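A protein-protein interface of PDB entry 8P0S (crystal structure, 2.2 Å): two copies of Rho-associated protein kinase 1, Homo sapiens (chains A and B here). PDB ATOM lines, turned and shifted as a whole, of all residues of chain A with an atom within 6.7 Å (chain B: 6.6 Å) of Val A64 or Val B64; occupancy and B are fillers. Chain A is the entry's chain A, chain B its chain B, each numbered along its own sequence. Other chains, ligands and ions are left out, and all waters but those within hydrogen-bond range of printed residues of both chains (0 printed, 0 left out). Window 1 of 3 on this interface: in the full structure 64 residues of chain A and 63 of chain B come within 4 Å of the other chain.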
ATOM      1  N   ASN A  59      20.816  35.154 -10.515  1.00  0.00           N
ATOM      2  CA  ASN A  59      20.245  33.823 -10.320  1.00  0.00           C
ATOM      3  C   ASN A  59      20.770  33.161  -9.048  1.00  0.00           C
ATOM      4  O   ASN A  59      20.011  32.547  -8.282  1.00  0.00           O
ATOM      5  CB  ASN A  59      20.560  32.971 -11.546  1.00  0.00           C
ATOM      6  CG  ASN A  59      19.509  31.947 -11.814  1.00  0.00           C
ATOM      7  OD1 ASN A  59      18.564  32.193 -12.567  1.00  0.00           O
ATOM      8  ND2 ASN A  59      19.645  30.787 -11.176  1.00  0.00           N
ATOM      9  N   LEU A  60      22.067  33.275  -8.791  1.00  0.00           N
ATOM     10  CA  LEU A  60      22.581  32.623  -7.614  1.00  0.00           C
ATOM     11  C   LEU A  60      22.129  33.334  -6.355  1.00  0.00           C
ATOM     12  O   LEU A  60      22.104  32.720  -5.288  1.00  0.00           O
ATOM     13  CB  LEU A  60      24.109  32.543  -7.659  1.00  0.00           C
ATOM     14  CG  LEU A  60      24.758  31.594  -8.668  1.00  0.00           C
ATOM     15  CD1 LEU A  60      26.219  31.963  -8.803  1.00  0.00           C
ATOM     16  CD2 LEU A  60      24.659  30.169  -8.203  1.00  0.00           C
ATOM     17  N   GLU A  61      21.842  34.635  -6.448  1.00  0.00           N
ATOM     18  CA  GLU A  61      21.334  35.371  -5.295  1.00  0.00           C
ATOM     19  C   GLU A  61      19.964  34.848  -4.892  1.00  0.00           C
ATOM     20  O   GLU A  61      19.670  34.704  -3.704  1.00  0.00           O
ATOM     21  CB  GLU A  61      21.234  36.870  -5.611  1.00  0.00           C
ATOM     22  CG  GLU A  61      22.464  37.676  -5.213  1.00  0.00           C
ATOM     23  CD  GLU A  61      22.311  39.176  -5.494  1.00  0.00           C
ATOM     24  OE1 GLU A  61      21.213  39.758  -5.275  1.00  0.00           O
ATOM     25  OE2 GLU A  61      23.300  39.773  -5.964  1.00  0.00           O
ATOM     26  N   SER A  62      19.111  34.569  -5.876  1.00  0.00           N
ATOM     27  CA  SER A  62      17.822  33.973  -5.584  1.00  0.00           C
ATOM     28  C   SER A  62      17.988  32.583  -5.024  1.00  0.00           C
ATOM     29  O   SER A  62      17.205  32.166  -4.170  1.00  0.00           O
ATOM     30  CB  SER A  62      16.979  33.922  -6.849  1.00  0.00           C
ATOM     31  OG  SER A  62      16.813  35.231  -7.304  1.00  0.00           O
ATOM     32  N   THR A  63      18.987  31.844  -5.497  1.00  0.00           N
ATOM     33  CA  THR A  63      19.172  30.508  -4.969  1.00  0.00           C
ATOM     34  C   THR A  63      19.550  30.598  -3.509  1.00  0.00           C
ATOM     35  O   THR A  63      19.065  29.822  -2.680  1.00  0.00           O
ATOM     36  CB  THR A  63      20.249  29.759  -5.759  1.00  0.00           C
ATOM     37  OG1 THR A  63      19.753  29.463  -7.072  1.00  0.00           O
ATOM     38  CG2 THR A  63      20.571  28.451  -5.076  1.00  0.00           C
ATOM     39  N   VAL A  64      20.381  31.577  -3.170  1.00  0.00           N
ATOM     40  CA  VAL A  64      20.818  31.711  -1.785  1.00  0.00           C
ATOM     41  C   VAL A  64      19.630  32.023  -0.882  1.00  0.00           C
ATOM     42  O   VAL A  64      19.460  31.389   0.156  1.00  0.00           O
ATOM     43  CB  VAL A  64      21.919  32.783  -1.675  1.00  0.00           C
ATOM     44  CG1 VAL A  64      22.257  33.054  -0.225  1.00  0.00           C
ATOM     45  CG2 VAL A  64      23.160  32.332  -2.440  1.00  0.00           C
ATOM     46  N   SER A  65      18.786  33.007  -1.266  1.00  0.00           N
ATOM     47  CA  SER A  65      17.615  33.343  -0.448  1.00  0.00           C
ATOM     48  C   SER A  65      16.727  32.138  -0.257  1.00  0.00           C
ATOM     49  O   SER A  65      16.248  31.869   0.852  1.00  0.00           O
ATOM     50  CB  SER A  65      16.800  34.475  -1.095  1.00  0.00           C
ATOM     51  OG  SER A  65      17.667  35.486  -1.494  1.00  0.00           O
ATOM     52  N   GLN A  66      16.496  31.394  -1.335  1.00  0.00           N
ATOM     53  CA  GLN A  66      15.642  30.220  -1.249  1.00  0.00           C
ATOM     54  C   GLN A  66      16.200  29.184  -0.271  1.00  0.00           C
ATOM     55  O   GLN A  66      15.462  28.651   0.566  1.00  0.00           O
ATOM     56  CB  GLN A  66      15.458  29.625  -2.649  1.00  0.00           C
ATOM     57  CG  GLN A  66      14.635  28.352  -2.683  1.00  0.00           C
ATOM     58  CD  GLN A  66      13.211  28.513  -2.135  1.00  0.00           C
ATOM     59  OE1 GLN A  66      12.583  29.570  -2.257  1.00  0.00           O
ATOM     60  NE2 GLN A  66      12.697  27.450  -1.553  1.00  0.00           N
ATOM     61  N   ILE A  67      17.502  28.882  -0.362  1.00  0.00           N
ATOM     62  CA  ILE A  67      18.095  27.804   0.436  1.00  0.00           C
ATOM     63  C   ILE A  67      18.178  28.194   1.897  1.00  0.00           C
ATOM     64  O   ILE A  67      18.063  27.339   2.785  1.00  0.00           O
ATOM     65  CB  ILE A  67      19.509  27.441  -0.054  1.00  0.00           C
ATOM     66  CG1 ILE A  67      19.529  26.756  -1.396  1.00  0.00           C
ATOM     67  CG2 ILE A  67      20.190  26.516   0.958  1.00  0.00           C
ATOM     68  CD1 ILE A  67      20.923  26.841  -1.982  1.00  0.00           C
ATOM     69  N   GLU A  68      18.484  29.466   2.177  1.00  0.00           N
ATOM     70  CA  GLU A  68      18.499  29.901   3.574  1.00  0.00           C
ATOM     71  C   GLU A  68      17.141  29.682   4.224  1.00  0.00           C
ATOM     72  O   GLU A  68      17.066  29.182   5.348  1.00  0.00           O
ATOM     73  CB  GLU A  68      18.914  31.363   3.668  1.00  0.00           C
ATOM     74  CG  GLU A  68      20.303  31.595   3.046  1.00  0.00           C
ATOM     75  CD  GLU A  68      21.191  32.527   3.829  1.00  0.00           C
ATOM     76  OE1 GLU A  68      20.885  33.748   3.882  1.00  0.00           O
ATOM     77  OE2 GLU A  68      22.216  32.034   4.359  1.00  0.00           O
ATOM     78  N   LYS A  69      16.055  30.023   3.514  1.00  0.00           N
ATOM     79  CA  LYS A  69      14.709  29.789   4.031  1.00  0.00           C
ATOM     80  C   LYS A  69      14.435  28.297   4.165  1.00  0.00           C
ATOM     81  O   LYS A  69      13.794  27.853   5.120  1.00  0.00           O
ATOM     82  CB  LYS A  69      13.651  30.419   3.103  1.00  0.00           C
ATOM     83  CG  LYS A  69      12.237  29.941   3.496  1.00  0.00           C
ATOM     84  CD  LYS A  69      11.161  29.969   2.425  1.00  0.00           C
ATOM     85  CE  LYS A  69      11.583  29.483   1.043  1.00  0.00           C
ATOM     86  NZ  LYS A  69      10.718  30.234   0.083  1.00  0.00           N
ATOM     87  N   ASN B  59      31.987  33.938  -6.078  1.00  0.00           N
ATOM     88  CA  ASN B  59      31.861  33.918  -4.629  1.00  0.00           C
ATOM     89  C   ASN B  59      30.544  33.267  -4.197  1.00  0.00           C
ATOM     90  O   ASN B  59      30.515  32.450  -3.265  1.00  0.00           O
ATOM     91  CB  ASN B  59      31.982  35.353  -4.104  1.00  0.00           C
ATOM     92  CG  ASN B  59      31.674  35.463  -2.635  1.00  0.00           C
ATOM     93  OD1 ASN B  59      32.184  34.678  -1.822  1.00  0.00           O
ATOM     94  ND2 ASN B  59      30.817  36.427  -2.272  1.00  0.00           N
ATOM     95  N   LEU B  60      29.445  33.612  -4.866  1.00  0.00           N
ATOM     96  CA  LEU B  60      28.148  33.042  -4.516  1.00  0.00           C
ATOM     97  C   LEU B  60      28.088  31.555  -4.844  1.00  0.00           C
ATOM     98  O   LEU B  60      27.292  30.818  -4.251  1.00  0.00           O
ATOM     99  CB  LEU B  60      27.051  33.781  -5.263  1.00  0.00           C
ATOM    100  CG  LEU B  60      26.691  35.175  -4.749  1.00  0.00           C
ATOM    101  CD1 LEU B  60      25.691  35.812  -5.669  1.00  0.00           C
ATOM    102  CD2 LEU B  60      26.148  35.107  -3.319  1.00  0.00           C
ATOM    103  N   GLU B  61      28.892  31.108  -5.808  1.00  0.00           N
ATOM    104  CA  GLU B  61      28.994  29.675  -6.073  1.00  0.00           C
ATOM    105  C   GLU B  61      29.521  28.961  -4.848  1.00  0.00           C
ATOM    106  O   GLU B  61      28.963  27.946  -4.408  1.00  0.00           O
ATOM    107  CB  GLU B  61      29.900  29.425  -7.264  1.00  0.00           C
ATOM    108  CG  GLU B  61      29.286  29.816  -8.608  1.00  0.00           C
ATOM    109  CD  GLU B  61      30.266  29.701  -9.785  1.00  0.00           C
ATOM    110  OE1 GLU B  61      31.485  29.511  -9.552  1.00  0.00           O
ATOM    111  OE2 GLU B  61      29.818  29.785 -10.953  1.00  0.00           O
ATOM    112  N   SER B  62      30.568  29.509  -4.248  1.00  0.00           N
ATOM    113  CA  SER B  62      31.048  28.942  -2.998  1.00  0.00           C
ATOM    114  C   SER B  62      29.971  28.988  -1.915  1.00  0.00           C
ATOM    115  O   SER B  62      29.766  28.000  -1.197  1.00  0.00           O
ATOM    116  CB  SER B  62      32.300  29.685  -2.558  1.00  0.00           C
ATOM    117  OG  SER B  62      33.054  28.846  -1.719  1.00  0.00           O
ATOM    118  N   THR B  63      29.260  30.119  -1.792  1.00  0.00           N
ATOM    119  CA  THR B  63      28.194  30.228  -0.785  1.00  0.00           C
ATOM    120  C   THR B  63      27.097  29.204  -1.024  1.00  0.00           C
ATOM    121  O   THR B  63      26.621  28.559  -0.090  1.00  0.00           O
ATOM    122  CB  THR B  63      27.575  31.628  -0.795  1.00  0.00           C
ATOM    123  OG1 THR B  63      28.602  32.589  -0.649  1.00  0.00           O
ATOM    124  CG2 THR B  63      26.487  31.818   0.322  1.00  0.00           C
ATOM    125  N   VAL B  64      26.641  29.084  -2.270  1.00  0.00           N
ATOM    126  CA  VAL B  64      25.618  28.094  -2.563  1.00  0.00           C
ATOM    127  C   VAL B  64      26.093  26.715  -2.128  1.00  0.00           C
ATOM    128  O   VAL B  64      25.402  25.990  -1.400  1.00  0.00           O
ATOM    129  CB  VAL B  64      25.265  28.121  -4.053  1.00  0.00           C
ATOM    130  CG1 VAL B  64      24.490  26.866  -4.418  1.00  0.00           C
ATOM    131  CG2 VAL B  64      24.464  29.356  -4.373  1.00  0.00           C
ATOM    132  N   SER B  65      27.311  26.354  -2.517  1.00  0.00           N
ATOM    133  CA  SER B  65      27.761  24.997  -2.249  1.00  0.00           C
ATOM    134  C   SER B  65      27.893  24.762  -0.752  1.00  0.00           C
ATOM    135  O   SER B  65      27.523  23.698  -0.240  1.00  0.00           O
ATOM    136  CB  SER B  65      29.078  24.725  -2.986  1.00  0.00           C
ATOM    137  OG  SER B  65      29.802  23.706  -2.330  1.00  0.00           O
ATOM    138  N   GLN B  66      28.358  25.763  -0.020  1.00  0.00           N
ATOM    139  CA  GLN B  66      28.470  25.580   1.417  1.00  0.00           C
ATOM    140  C   GLN B  66      27.103  25.556   2.105  1.00  0.00           C
ATOM    141  O   GLN B  66      26.937  24.841   3.101  1.00  0.00           O
ATOM    142  CB  GLN B  66      29.375  26.661   2.013  1.00  0.00           C
ATOM    143  CG  GLN B  66      29.503  26.628   3.539  1.00  0.00           C
ATOM    144  CD  GLN B  66      29.958  25.273   4.115  1.00  0.00           C
ATOM    145  OE1 GLN B  66      30.577  24.448   3.426  1.00  0.00           O
ATOM    146  NE2 GLN B  66      29.619  25.036   5.383  1.00  0.00           N
ATOM    147  N   ILE B  67      26.105  26.302   1.615  1.00  0.00           N
ATOM    148  CA  ILE B  67      24.823  26.173   2.313  1.00  0.00           C
ATOM    149  C   ILE B  67      24.032  24.960   1.823  1.00  0.00           C
ATOM    150  O   ILE B  67      23.234  24.402   2.578  1.00  0.00           O
ATOM    151  CB  ILE B  67      23.973  27.457   2.249  1.00  0.00           C
ATOM    152  CG1 ILE B  67      23.604  27.849   0.837  1.00  0.00           C
ATOM    153  CG2 ILE B  67      24.663  28.589   2.924  1.00  0.00           C
ATOM    154  CD1 ILE B  67      23.026  29.286   0.795  1.00  0.00           C
ATOM    155  N   GLU B  68      24.218  24.524   0.575  1.00  0.00           N
ATOM    156  CA  GLU B  68      23.603  23.262   0.167  1.00  0.00           C
ATOM    157  C   GLU B  68      24.107  22.117   1.024  1.00  0.00           C
ATOM    158  O   GLU B  68      23.337  21.206   1.375  1.00  0.00           O
ATOM    159  CB  GLU B  68      23.866  22.949  -1.309  1.00  0.00           C
ATOM    160  CG  GLU B  68      23.155  23.841  -2.278  1.00  0.00           C
ATOM    161  CD  GLU B  68      21.738  23.332  -2.608  1.00  0.00           C
ATOM    162  OE1 GLU B  68      20.954  23.028  -1.662  1.00  0.00           O
ATOM    163  OE2 GLU B  68      21.403  23.239  -3.813  1.00  0.00           O
ATOM    164  N   LYS B  69      25.398  22.145   1.368  1.00  0.00           N
ATOM    165  CA  LYS B  69      25.942  21.144   2.271  1.00  0.00           C
ATOM    166  C   LYS B  69      25.233  21.184   3.614  1.00  0.00           C
ATOM    167  O   LYS B  69      24.854  20.140   4.148  1.00  0.00           O
ATOM    168  CB  LYS B  69      27.442  21.338   2.460  1.00  0.00           C
ATOM    169  CG  LYS B  69      28.109  20.182   3.203  1.00  0.00           C
ATOM    170  CD  LYS B  69      28.342  20.477   4.690  1.00  0.00           C
ATOM    171  CE  LYS B  69      29.375  19.523   5.324  1.00  0.00           C
ATOM    172  NZ  LYS B  69      28.863  18.113   5.410  1.00  0.00           N
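The backbone carbonyl oxygen (O) of Glu A61 sits at hydrogen-bond distance from the side-chain hydroxyl (OG) of Ser A65 (3.1 Å).
Leu B60 touches Leu A60 (CB to CB, 3.99 Å).
Glu B61 touches Leu A60 (CG to CD1, 3.7 Å).
Leu A60 touches Val B64.
CG of Glu A61 touches CD1 of Leu B60, at 3.8 Å.
Val A64 touches Val B64.
Val A64 touches Ile B67.
Ile A67 touches Ile B67 (CG2 to CG1, 3.7 Å).
CD of Glu B68 touches CD1 of Ile A67 (3.7 Å).
Of the 11 printed residues of chain B, 5 touch a printed residue of chain A.
Among the printed residues, 8 pairs touch across the chains.
Among the printed residues, no Asp or Glu carboxylate lies within 4 Å of a Lys or Arg side-chain nitrogen of the other chain.
Of the printed residues of chain B, Leu A60 touches Leu B60 (3.99 Å), Glu B61 (3.7 Å) and Val B64 (3.9 Å).
Of the printed residues of chain B, Glu A61 touches Leu B60 (3.8 Å).
Thr A63 touches none of the printed residues of chain B.
Of chain B, only Val B64 (3.8 Å) and Ile B67 (3.98 Å) come within 4 Å of Val A64.
Of the printed residues of chain A, Leu B60 touches Leu A60 and Glu A61.
Thr B63 touches none of the printed residues of chain A.
Val B64 touches two residues of chain A.
Of the printed residues of chain A, Ile B67 touches Val A64 (3.98 Å) and Ile A67 (3.7 Å).
The nearest residue of chain B that does not touch Val A64 is Leu B60 (4.2 Å).
The nearest printed residue of chain A that does not touch Leu B60 is Val A64 (4.2 Å).
Leu A60 touches its own counterpart, Leu B60.
Val A64 touches its own counterpart, Val B64.
Ile B67 touches its own counterpart, Ile A67.
Ile A67 touches Glu B68, but with the chains exchanged Glu A68 does not touch Ile B67 (4.2 Å).
Of the 8 pairs that touch across the chains among the printed residues, 5 have their exchanged pair printed and touching as well.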
